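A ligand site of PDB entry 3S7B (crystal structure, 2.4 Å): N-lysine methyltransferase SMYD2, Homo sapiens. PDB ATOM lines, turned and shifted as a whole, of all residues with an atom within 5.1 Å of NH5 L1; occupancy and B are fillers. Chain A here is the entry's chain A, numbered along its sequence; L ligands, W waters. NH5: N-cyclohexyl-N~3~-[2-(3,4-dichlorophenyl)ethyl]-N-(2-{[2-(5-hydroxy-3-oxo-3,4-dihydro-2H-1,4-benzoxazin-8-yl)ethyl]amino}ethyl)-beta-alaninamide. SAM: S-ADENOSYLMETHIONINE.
Merely in contact with NH5 L1: Thr 105, Leu 141, Lys 145, Ile 149, Ala 177, Val 179, Cys 181, Asn 182, Phe 184, Thr 185, Ser 196, Ala 203, Thr 238, Ser 239, Tyr 240, Ser 257 and Phe 259.
Hydrophobic or aromatic side chains within 4 Å of NH5 L1: Leu 141, Ile 149, Phe 184, Ala 203, Tyr 240, Tyr 258 and Phe 259.
20 residues have an atom within 4 Å of NH5 L1: Thr 105, Leu 141, Lys 145, Ile 149, Ala 177, Val 179, Asn 180, Cys 181, Asn 182, Gly 183, Phe 184, Thr 185, Ser 196, Ala 203, Thr 238, Ser 239, Tyr 240, Ser 257, Tyr 258 and Phe 259.
The nearest printed residue that does not touch NH5 L1 is Asp 256 (4.04 Å).
The backbone carbonyl oxygen (O) of Phe 176 is in hydrogen-bond range of the side-chain amide nitrogen (ND2) of Asn 180, at 2.7 Å.
OH of Tyr 240 lies within hydrogen-bond range of O of Met 205 (2.6 Å).
ND2 of Asn 182 lies close to SG of Cys 181 (3.8 Å).
The side-chain amino group (NZ) of Lys 145 is in salt-bridge range of the side-chain carboxylate (OD1) of Asp 256, at 3.0 Å.
O of Gly 183 sits at hydrogen-bond distance from N17 of NH5 L1.
O26 of NH5 L1 lies close to OH of Tyr 258, at 3.2 Å.
The side-chain amide oxygen of Asn 180 lies within hydrogen-bond range of a nitrogen (N9) of NH5 L1, 3.3 Å away.
O3' of SAM L2 lies within hydrogen-bond range of O of Tyr 258.
SG of Cys 181 is in hydrogen-bond range of O3' of SAM L2 (3.5 Å).
Water W2 lies within hydrogen-bond range of O31 of NH5 L1 (2.6 Å), O of Val 202 (2.7 Å) and O of Met 205 (2.9 Å).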
ATOM      1  N   THR A 105     -13.531   2.439  15.958  1.00  0.00           N
ATOM      2  CA  THR A 105     -12.487   2.216  14.944  1.00  0.00           C
ATOM      3  C   THR A 105     -13.094   2.304  13.521  1.00  0.00           C
ATOM      4  O   THR A 105     -12.491   2.918  12.624  1.00  0.00           O
ATOM      5  CB  THR A 105     -11.852   0.820  15.128  1.00  0.00           C
ATOM      6  OG1 THR A 105     -11.529   0.583  16.477  1.00  0.00           O
ATOM      7  CG2 THR A 105     -10.708   0.574  14.172  1.00  0.00           C
ATOM      8  N   LEU A 108     -14.132   5.947  12.807  1.00  0.00           N
ATOM      9  CA  LEU A 108     -12.940   6.707  12.422  1.00  0.00           C
ATOM     10  C   LEU A 108     -12.467   6.327  11.009  1.00  0.00           C
ATOM     11  O   LEU A 108     -12.112   7.217  10.221  1.00  0.00           O
ATOM     12  CB  LEU A 108     -11.791   6.553  13.441  1.00  0.00           C
ATOM     13  CG  LEU A 108     -10.509   7.401  13.191  1.00  0.00           C
ATOM     14  CD1 LEU A 108     -10.820   8.925  13.136  1.00  0.00           C
ATOM     15  CD2 LEU A 108      -9.453   7.125  14.252  1.00  0.00           C
ATOM     16  N   LEU A 141       0.241  -9.950  11.695  1.00  0.00           N
ATOM     17  CA  LEU A 141      -1.137 -10.231  12.078  1.00  0.00           C
ATOM     18  C   LEU A 141      -1.397 -11.733  12.290  1.00  0.00           C
ATOM     19  O   LEU A 141      -1.115 -12.544  11.390  1.00  0.00           O
ATOM     20  CB  LEU A 141      -2.090  -9.680  10.970  1.00  0.00           C
ATOM     21  CG  LEU A 141      -2.806  -8.331  11.137  1.00  0.00           C
ATOM     22  CD1 LEU A 141      -1.986  -7.283  11.898  1.00  0.00           C
ATOM     23  CD2 LEU A 141      -3.211  -7.778   9.787  1.00  0.00           C
ATOM     24  N   LYS A 145      -6.314 -11.346  15.200  1.00  0.00           N
ATOM     25  CA  LYS A 145      -6.294  -9.977  14.713  1.00  0.00           C
ATOM     26  C   LYS A 145      -6.918  -9.840  13.332  1.00  0.00           C
ATOM     27  O   LYS A 145      -7.698  -8.909  13.105  1.00  0.00           O
ATOM     28  CB  LYS A 145      -4.881  -9.356  14.790  1.00  0.00           C
ATOM     29  CG  LYS A 145      -4.546  -8.832  16.182  1.00  0.00           C
ATOM     30  CD  LYS A 145      -3.100  -8.340  16.248  1.00  0.00           C
ATOM     31  CE  LYS A 145      -2.763  -7.723  17.579  1.00  0.00           C
ATOM     32  NZ  LYS A 145      -2.346  -8.727  18.580  1.00  0.00           N
ATOM     33  N   LEU A 148     -10.672  -9.975  13.784  1.00  0.00           N
ATOM     34  CA  LEU A 148     -11.183  -8.720  14.329  1.00  0.00           C
ATOM     35  C   LEU A 148     -11.268  -7.662  13.218  1.00  0.00           C
ATOM     36  O   LEU A 148     -12.301  -6.982  13.095  1.00  0.00           O
ATOM     37  CB  LEU A 148     -10.371  -8.222  15.530  1.00  0.00           C
ATOM     38  CG  LEU A 148     -10.557  -8.990  16.833  1.00  0.00           C
ATOM     39  CD1 LEU A 148      -9.323  -8.882  17.731  1.00  0.00           C
ATOM     40  CD2 LEU A 148     -11.812  -8.536  17.572  1.00  0.00           C
ATOM     41  N   ILE A 149     -10.219  -7.567  12.376  1.00  0.00           N
ATOM     42  CA  ILE A 149     -10.162  -6.665  11.227  1.00  0.00           C
ATOM     43  C   ILE A 149     -11.296  -7.027  10.208  1.00  0.00           C
ATOM     44  O   ILE A 149     -11.948  -6.125   9.658  1.00  0.00           O
ATOM     45  CB  ILE A 149      -8.747  -6.628  10.587  1.00  0.00           C
ATOM     46  CG1 ILE A 149      -7.725  -5.897  11.518  1.00  0.00           C
ATOM     47  CG2 ILE A 149      -8.768  -5.990   9.188  1.00  0.00           C
ATOM     48  CD1 ILE A 149      -6.286  -5.997  11.098  1.00  0.00           C
ATOM     49  N   PHE A 176      -7.160  -0.776   8.361  1.00  0.00           N
ATOM     50  CA  PHE A 176      -7.553  -1.071   9.740  1.00  0.00           C
ATOM     51  C   PHE A 176      -6.323  -1.337  10.612  1.00  0.00           C
ATOM     52  O   PHE A 176      -6.270  -0.852  11.748  1.00  0.00           O
ATOM     53  CB  PHE A 176      -8.588  -2.227   9.806  1.00  0.00           C
ATOM     54  CG  PHE A 176     -10.010  -1.720   9.635  1.00  0.00           C
ATOM     55  CD1 PHE A 176     -10.647  -1.022  10.654  1.00  0.00           C
ATOM     56  CD2 PHE A 176     -10.680  -1.884   8.415  1.00  0.00           C
ATOM     57  CE1 PHE A 176     -11.947  -0.516  10.478  1.00  0.00           C
ATOM     58  CE2 PHE A 176     -11.983  -1.382   8.252  1.00  0.00           C
ATOM     59  CZ  PHE A 176     -12.601  -0.695   9.282  1.00  0.00           C
ATOM     60  N   ALA A 177      -5.294  -2.035  10.069  1.00  0.00           N
ATOM     61  CA  ALA A 177      -4.064  -2.288  10.796  1.00  0.00           C
ATOM     62  C   ALA A 177      -3.275  -0.989  11.035  1.00  0.00           C
ATOM     63  O   ALA A 177      -2.763  -0.790  12.126  1.00  0.00           O
ATOM     64  CB  ALA A 177      -3.212  -3.350  10.076  1.00  0.00           C
ATOM     65  N   VAL A 179      -4.581   2.056  11.270  1.00  0.00           N
ATOM     66  CA  VAL A 179      -5.414   2.778  12.246  1.00  0.00           C
ATOM     67  C   VAL A 179      -5.129   2.280  13.669  1.00  0.00           C
ATOM     68  O   VAL A 179      -4.978   3.099  14.557  1.00  0.00           O
ATOM     69  CB  VAL A 179      -6.923   2.755  11.860  1.00  0.00           C
ATOM     70  CG1 VAL A 179      -7.822   3.297  12.977  1.00  0.00           C
ATOM     71  CG2 VAL A 179      -7.157   3.516  10.574  1.00  0.00           C
ATOM     72  N   ASN A 180      -5.007   0.951  13.888  1.00  0.00           N
ATOM     73  CA  ASN A 180      -4.673   0.398  15.205  1.00  0.00           C
ATOM     74  C   ASN A 180      -3.256   0.763  15.635  1.00  0.00           C
ATOM     75  O   ASN A 180      -3.047   1.056  16.819  1.00  0.00           O
ATOM     76  CB  ASN A 180      -4.875  -1.104  15.240  1.00  0.00           C
ATOM     77  CG  ASN A 180      -6.348  -1.426  15.329  1.00  0.00           C
ATOM     78  OD1 ASN A 180      -6.988  -1.289  16.381  1.00  0.00           O
ATOM     79  ND2 ASN A 180      -6.963  -1.709  14.180  1.00  0.00           N
ATOM     80  N   CYS A 181      -2.325   0.804  14.669  1.00  0.00           N
ATOM     81  CA  CYS A 181      -0.932   1.135  14.920  1.00  0.00           C
ATOM     82  C   CYS A 181      -0.681   2.616  15.188  1.00  0.00           C
ATOM     83  O   CYS A 181       0.222   2.965  15.954  1.00  0.00           O
ATOM     84  CB  CYS A 181      -0.063   0.634  13.760  1.00  0.00           C
ATOM     85  SG  CYS A 181       1.718   0.812  14.019  1.00  0.00           S
ATOM     86  N   ASN A 182      -1.469   3.492  14.517  1.00  0.00           N
ATOM     87  CA  ASN A 182      -1.253   4.922  14.516  1.00  0.00           C
ATOM     88  C   ASN A 182      -2.342   5.817  15.077  1.00  0.00           C
ATOM     89  O   ASN A 182      -2.114   7.033  15.194  1.00  0.00           O
ATOM     90  CB  ASN A 182      -0.844   5.370  13.096  1.00  0.00           C
ATOM     91  CG  ASN A 182       0.391   4.672  12.586  1.00  0.00           C
ATOM     92  OD1 ASN A 182       1.509   5.075  12.878  1.00  0.00           O
ATOM     93  ND2 ASN A 182       0.208   3.564  11.900  1.00  0.00           N
ATOM     94  N   GLY A 183      -3.494   5.243  15.393  1.00  0.00           N
ATOM     95  CA  GLY A 183      -4.633   5.991  15.923  1.00  0.00           C
ATOM     96  C   GLY A 183      -4.444   6.482  17.346  1.00  0.00           C
ATOM     97  O   GLY A 183      -3.761   5.849  18.171  1.00  0.00           O
ATOM     98  N   PHE A 184      -5.067   7.618  17.635  1.00  0.00           N
ATOM     99  CA  PHE A 184      -5.010   8.239  18.948  1.00  0.00           C
ATOM    100  C   PHE A 184      -6.377   8.298  19.608  1.00  0.00           C
ATOM    101  O   PHE A 184      -7.392   8.482  18.940  1.00  0.00           O
ATOM    102  CB  PHE A 184      -4.481   9.692  18.828  1.00  0.00           C
ATOM    103  CG  PHE A 184      -3.011   9.815  18.524  1.00  0.00           C
ATOM    104  CD1 PHE A 184      -2.086  10.063  19.531  1.00  0.00           C
ATOM    105  CD2 PHE A 184      -2.548   9.731  17.207  1.00  0.00           C
ATOM    106  CE1 PHE A 184      -0.724  10.210  19.229  1.00  0.00           C
ATOM    107  CE2 PHE A 184      -1.193   9.867  16.906  1.00  0.00           C
ATOM    108  CZ  PHE A 184      -0.285  10.100  17.918  1.00  0.00           C
ATOM    109  N   THR A 185      -6.387   8.253  20.918  1.00  0.00           N
ATOM    110  CA  THR A 185      -7.559   8.488  21.725  1.00  0.00           C
ATOM    111  C   THR A 185      -7.438   9.950  22.123  1.00  0.00           C
ATOM    112  O   THR A 185      -6.362  10.384  22.569  1.00  0.00           O
ATOM    113  CB  THR A 185      -7.493   7.639  23.008  1.00  0.00           C
ATOM    114  OG1 THR A 185      -7.645   6.269  22.705  1.00  0.00           O
ATOM    115  CG2 THR A 185      -8.494   8.088  24.064  1.00  0.00           C
ATOM    116  N   SER A 196     -11.630   9.523  19.070  1.00  0.00           N
ATOM    117  CA  SER A 196     -10.504   8.919  18.374  1.00  0.00           C
ATOM    118  C   SER A 196     -10.146   9.774  17.186  1.00  0.00           C
ATOM    119  O   SER A 196     -11.013  10.443  16.634  1.00  0.00           O
ATOM    120  CB  SER A 196     -10.857   7.505  17.944  1.00  0.00           C
ATOM    121  OG  SER A 196     -10.991   6.692  19.107  1.00  0.00           O
ATOM    122  N   VAL A 202       2.146  13.400  14.477  1.00  0.00           N
ATOM    123  CA  VAL A 202       2.318  12.977  15.872  1.00  0.00           C
ATOM    124  C   VAL A 202       2.637  11.463  15.903  1.00  0.00           C
ATOM    125  O   VAL A 202       3.409  11.027  16.751  1.00  0.00           O
ATOM    126  CB  VAL A 202       1.078  13.350  16.745  1.00  0.00           C
ATOM    127  CG1 VAL A 202       1.305  13.023  18.202  1.00  0.00           C
ATOM    128  CG2 VAL A 202       0.729  14.823  16.594  1.00  0.00           C
ATOM    129  N   ALA A 203       2.066  10.689  14.963  1.00  0.00           N
ATOM    130  CA  ALA A 203       2.282   9.237  14.877  1.00  0.00           C
ATOM    131  C   ALA A 203       3.699   8.863  14.406  1.00  0.00           C
ATOM    132  O   ALA A 203       4.095   7.701  14.535  1.00  0.00           O
ATOM    133  CB  ALA A 203       1.221   8.577  14.006  1.00  0.00           C
ATOM    134  N   MET A 205       6.309   9.871  15.968  1.00  0.00           N
ATOM    135  CA  MET A 205       7.065   9.641  17.203  1.00  0.00           C
ATOM    136  C   MET A 205       7.034   8.223  17.707  1.00  0.00           C
ATOM    137  O   MET A 205       5.969   7.612  17.810  1.00  0.00           O
ATOM    138  CB  MET A 205       6.681  10.624  18.319  1.00  0.00           C
ATOM    139  CG  MET A 205       6.928  12.073  17.964  1.00  0.00           C
ATOM    140  SD  MET A 205       6.503  13.175  19.323  1.00  0.00           S
ATOM    141  CE  MET A 205       4.666  13.100  19.286  1.00  0.00           C
ATOM    142  N   VAL A 215       1.717  14.292  24.712  1.00  0.00           N
ATOM    143  CA  VAL A 215       0.704  14.743  23.761  1.00  0.00           C
ATOM    144  C   VAL A 215      -0.559  15.172  24.543  1.00  0.00           C
ATOM    145  O   VAL A 215      -1.071  14.423  25.376  1.00  0.00           O
ATOM    146  CB  VAL A 215       0.362  13.660  22.703  1.00  0.00           C
ATOM    147  CG1 VAL A 215      -0.704  14.175  21.725  1.00  0.00           C
ATOM    148  CG2 VAL A 215       1.617  13.173  21.968  1.00  0.00           C
ATOM    149  N   THR A 238       7.444   9.625  22.990  1.00  0.00           N
ATOM    150  CA  THR A 238       6.231   9.749  23.758  1.00  0.00           C
ATOM    151  C   THR A 238       5.980   8.322  24.349  1.00  0.00           C
ATOM    152  O   THR A 238       6.616   7.358  23.921  1.00  0.00           O
ATOM    153  CB  THR A 238       5.127  10.289  22.816  1.00  0.00           C
ATOM    154  OG1 THR A 238       4.061  10.805  23.588  1.00  0.00           O
ATOM    155  CG2 THR A 238       4.652   9.276  21.808  1.00  0.00           C
ATOM    156  N   SER A 239       5.091   8.198  25.331  1.00  0.00           N
ATOM    157  CA  SER A 239       4.710   6.885  25.831  1.00  0.00           C
ATOM    158  C   SER A 239       3.385   6.520  25.172  1.00  0.00           C
ATOM    159  O   SER A 239       2.433   7.319  25.184  1.00  0.00           O
ATOM    160  CB  SER A 239       4.571   6.862  27.349  1.00  0.00           C
ATOM    161  OG  SER A 239       4.097   5.577  27.708  1.00  0.00           O
ATOM    162  N   TYR A 240       3.321   5.308  24.608  1.00  0.00           N
ATOM    163  CA  TYR A 240       2.120   4.769  23.961  1.00  0.00           C
ATOM    164  C   TYR A 240       1.183   4.114  24.995  1.00  0.00           C
ATOM    165  O   TYR A 240       0.042   3.813  24.669  1.00  0.00           O
ATOM    166  CB  TYR A 240       2.523   3.650  22.952  1.00  0.00           C
ATOM    167  CG  TYR A 240       3.265   4.057  21.697  1.00  0.00           C
ATOM    168  CD1 TYR A 240       3.677   5.383  21.482  1.00  0.00           C
ATOM    169  CD2 TYR A 240       3.592   3.121  20.712  1.00  0.00           C
ATOM    170  CE1 TYR A 240       4.406   5.750  20.350  1.00  0.00           C
ATOM    171  CE2 TYR A 240       4.278   3.479  19.554  1.00  0.00           C
ATOM    172  CZ  TYR A 240       4.702   4.801  19.389  1.00  0.00           C
ATOM    173  OH  TYR A 240       5.341   5.172  18.235  1.00  0.00           O
ATOM    174  N   ASP A 256       1.727  -6.964  22.044  1.00  0.00           N
ATOM    175  CA  ASP A 256       0.361  -7.229  21.589  1.00  0.00           C
ATOM    176  C   ASP A 256      -0.246  -6.105  20.723  1.00  0.00           C
ATOM    177  O   ASP A 256      -0.823  -6.403  19.677  1.00  0.00           O
ATOM    178  CB  ASP A 256      -0.550  -7.553  22.800  1.00  0.00           C
ATOM    179  CG  ASP A 256      -1.933  -8.069  22.399  1.00  0.00           C
ATOM    180  OD1 ASP A 256      -1.982  -9.020  21.578  1.00  0.00           O
ATOM    181  OD2 ASP A 256      -2.950  -7.530  22.911  1.00  0.00           O
ATOM    182  N   SER A 257      -0.134  -4.837  21.127  1.00  0.00           N
ATOM    183  CA  SER A 257      -0.758  -3.745  20.354  1.00  0.00           C
ATOM    184  C   SER A 257       0.134  -3.090  19.296  1.00  0.00           C
ATOM    185  O   SER A 257      -0.375  -2.551  18.316  1.00  0.00           O
ATOM    186  CB  SER A 257      -1.333  -2.670  21.279  1.00  0.00           C
ATOM    187  OG  SER A 257      -2.252  -3.201  22.229  1.00  0.00           O
ATOM    188  N   TYR A 258       1.470  -3.108  19.519  1.00  0.00           N
ATOM    189  CA  TYR A 258       2.435  -2.414  18.651  1.00  0.00           C
ATOM    190  C   TYR A 258       3.522  -3.254  18.047  1.00  0.00           C
ATOM    191  O   TYR A 258       4.342  -2.718  17.308  1.00  0.00           O
ATOM    192  CB  TYR A 258       2.958  -1.118  19.311  1.00  0.00           C
ATOM    193  CG  TYR A 258       1.847  -0.161  19.657  1.00  0.00           C
ATOM    194  CD1 TYR A 258       1.205   0.583  18.665  1.00  0.00           C
ATOM    195  CD2 TYR A 258       1.363  -0.057  20.967  1.00  0.00           C
ATOM    196  CE1 TYR A 258       0.126   1.418  18.978  1.00  0.00           C
ATOM    197  CE2 TYR A 258       0.279   0.756  21.278  1.00  0.00           C
ATOM    198  CZ  TYR A 258      -0.339   1.494  20.284  1.00  0.00           C
ATOM    199  OH  TYR A 258      -1.403   2.287  20.603  1.00  0.00           O
ATOM    200  N   PHE A 259       3.509  -4.562  18.304  1.00  0.00           N
ATOM    201  CA  PHE A 259       4.428  -5.556  17.704  1.00  0.00           C
ATOM    202  C   PHE A 259       5.917  -5.279  17.905  1.00  0.00           C
ATOM    203  O   PHE A 259       6.720  -5.535  17.016  1.00  0.00           O
ATOM    204  CB  PHE A 259       4.084  -5.799  16.221  1.00  0.00           C
ATOM    205  CG  PHE A 259       2.625  -6.041  15.955  1.00  0.00           C
ATOM    206  CD1 PHE A 259       2.101  -7.341  15.958  1.00  0.00           C
ATOM    207  CD2 PHE A 259       1.767  -4.984  15.658  1.00  0.00           C
ATOM    208  CE1 PHE A 259       0.739  -7.568  15.693  1.00  0.00           C
ATOM    209  CE2 PHE A 259       0.405  -5.211  15.393  1.00  0.00           C
ATOM    210  CZ  PHE A 259      -0.104  -6.493  15.415  1.00  0.00           C
HETATM  211  C1  NH5 L   1      -3.470  -4.082  17.692  1.00  0.00           C
HETATM  212  C2  NH5 L   1      -3.294  -4.170  16.313  1.00  0.00           C
HETATM  213  C3  NH5 L   1      -4.339  -4.650  15.520  1.00  0.00           C
HETATM  214  C4  NH5 L   1      -5.553  -5.031  16.106  1.00  0.00           C
HETATM  215  C5  NH5 L   1      -5.723  -4.931  17.484  1.00  0.00           C
HETATM  216  C6  NH5 L   1      -4.671  -4.462  18.283  1.00  0.00           C
HETATM  217  C7  NH5 L   1      -4.839  -4.378  19.782  1.00  0.00           C
HETATM  218  C8  NH5 L   1      -5.507  -3.090  20.277  1.00  0.00           C
HETATM  219  N9  NH5 L   1      -5.521  -2.018  19.259  1.00  0.00           N
HETATM  220  C10 NH5 L   1      -4.733  -0.868  19.705  1.00  0.00           C
HETATM  221  C11 NH5 L   1      -5.451   0.405  19.226  1.00  0.00           C
HETATM  222  C12 NH5 L   1      -5.472   1.486  20.307  1.00  0.00           C
HETATM  223  O13 NH5 L   1      -4.839   1.333  21.336  1.00  0.00           O
HETATM  224  N14 NH5 L   1      -6.176   2.621  20.076  1.00  0.00           N
HETATM  225  C15 NH5 L   1      -6.298   3.707  21.060  1.00  0.00           C
HETATM  226  C16 NH5 L   1      -4.975   4.084  21.746  1.00  0.00           C
HETATM  227  N17 NH5 L   1      -4.196   5.065  20.981  1.00  0.00           N
HETATM  228  C18 NH5 L   1      -3.241   5.767  21.870  1.00  0.00           C
HETATM  229  C19 NH5 L   1      -1.868   5.091  22.050  1.00  0.00           C
HETATM  230  C20 NH5 L   1      -0.782   6.097  21.741  1.00  0.00           C
HETATM  231  C21 NH5 L   1      -0.393   7.074  22.682  1.00  0.00           C
HETATM  232  C22 NH5 L   1       0.610   8.016  22.400  1.00  0.00           C
HETATM  233  C23 NH5 L   1       1.210   8.003  21.132  1.00  0.00           C
HETATM  234  C24 NH5 L   1       0.843   7.022  20.214  1.00  0.00           C
HETATM  235  C25 NH5 L   1      -0.153   6.118  20.512  1.00  0.00           C
HETATM  236  O26 NH5 L   1      -0.574   5.243  19.565  1.00  0.00           O
HETATM  237  C27 NH5 L   1      -0.579   5.725  18.202  1.00  0.00           C
HETATM  238  C28 NH5 L   1       0.676   6.500  17.868  1.00  0.00           C
HETATM  239  O29 NH5 L   1       1.086   6.605  16.736  1.00  0.00           O
HETATM  240  N30 NH5 L   1       1.315   7.066  18.898  1.00  0.00           N
HETATM  241  O31 NH5 L   1       2.155   8.885  20.706  1.00  0.00           O
HETATM  242  C32 NH5 L   1      -6.977   2.785  18.826  1.00  0.00           C
HETATM  243  C33 NH5 L   1      -8.453   2.351  19.040  1.00  0.00           C
HETATM  244  C34 NH5 L   1      -9.279   2.477  17.760  1.00  0.00           C
HETATM  245  C35 NH5 L   1      -9.205   3.905  17.179  1.00  0.00           C
HETATM  246  C36 NH5 L   1      -7.746   4.364  16.945  1.00  0.00           C
HETATM  247  C37 NH5 L   1      -6.890   4.194  18.211  1.00  0.00           C
HETATM  248 CL38 NH5 L   1      -6.876  -5.639  15.138  1.00  0.00          CL
HETATM  249 CL39 NH5 L   1      -4.158  -4.727  13.798  1.00  0.00          CL
HETATM  250  N   SAM L   2       8.558   4.039  13.717  1.00  0.00           N
HETATM  251  CA  SAM L   2       7.184   4.243  13.144  1.00  0.00           C
HETATM  252  C   SAM L   2       7.186   4.342  11.621  1.00  0.00           C
HETATM  253  O   SAM L   2       6.141   4.592  11.029  1.00  0.00           O
HETATM  254  OXT SAM L   2       8.226   4.161  10.984  1.00  0.00           O
HETATM  255  CB  SAM L   2       6.494   5.489  13.765  1.00  0.00           C
HETATM  256  CG  SAM L   2       5.762   5.174  15.105  1.00  0.00           C
HETATM  257  SD  SAM L   2       4.291   4.118  14.763  1.00  0.00           S
HETATM  258  CE  SAM L   2       2.931   4.913  15.541  1.00  0.00           C
HETATM  259  C5' SAM L   2       4.396   2.732  15.881  1.00  0.00           C
HETATM  260  C4' SAM L   2       5.441   1.686  15.377  1.00  0.00           C
HETATM  261  O4' SAM L   2       6.797   2.162  15.485  1.00  0.00           O
HETATM  262  C3' SAM L   2       5.402   0.473  16.309  1.00  0.00           C
HETATM  263  O3' SAM L   2       4.331  -0.403  16.068  1.00  0.00           O
HETATM  264  C2' SAM L   2       6.807  -0.134  16.145  1.00  0.00           C
HETATM  265  O2' SAM L   2       6.940  -0.841  14.899  1.00  0.00           O
HETATM  266  C1' SAM L   2       7.654   1.145  16.065  1.00  0.00           C
HETATM  267  N9  SAM L   2       8.183   1.607  17.344  1.00  0.00           N
HETATM  268  C8  SAM L   2       7.714   2.689  18.126  1.00  0.00           C
HETATM  269  N7  SAM L   2       8.466   2.772  19.171  1.00  0.00           N
HETATM  270  C5  SAM L   2       9.427   1.784  19.157  1.00  0.00           C
HETATM  271  C6  SAM L   2      10.503   1.394  20.010  1.00  0.00           C
HETATM  272  N6  SAM L   2      10.774   2.054  21.167  1.00  0.00           N
HETATM  273  N1  SAM L   2      11.268   0.273  19.641  1.00  0.00           N
HETATM  274  C2  SAM L   2      11.016  -0.431  18.499  1.00  0.00           C
HETATM  275  N3  SAM L   2      10.037  -0.065  17.671  1.00  0.00           N
HETATM  276  C4  SAM L   2       9.244   1.024  17.955  1.00  0.00           C
HETATM  277  O   HOH W   1      -1.368  -2.749  13.432  1.00  0.00           O
HETATM  278  O   HOH W   2       3.395   8.853  18.413  1.00  0.00           O
HETATM  279  O   HOH W   3      -2.858   3.237  18.697  1.00  0.00           O
HETATM  280  O   HOH W   4      -3.926   8.747  22.599  1.00  0.00           O
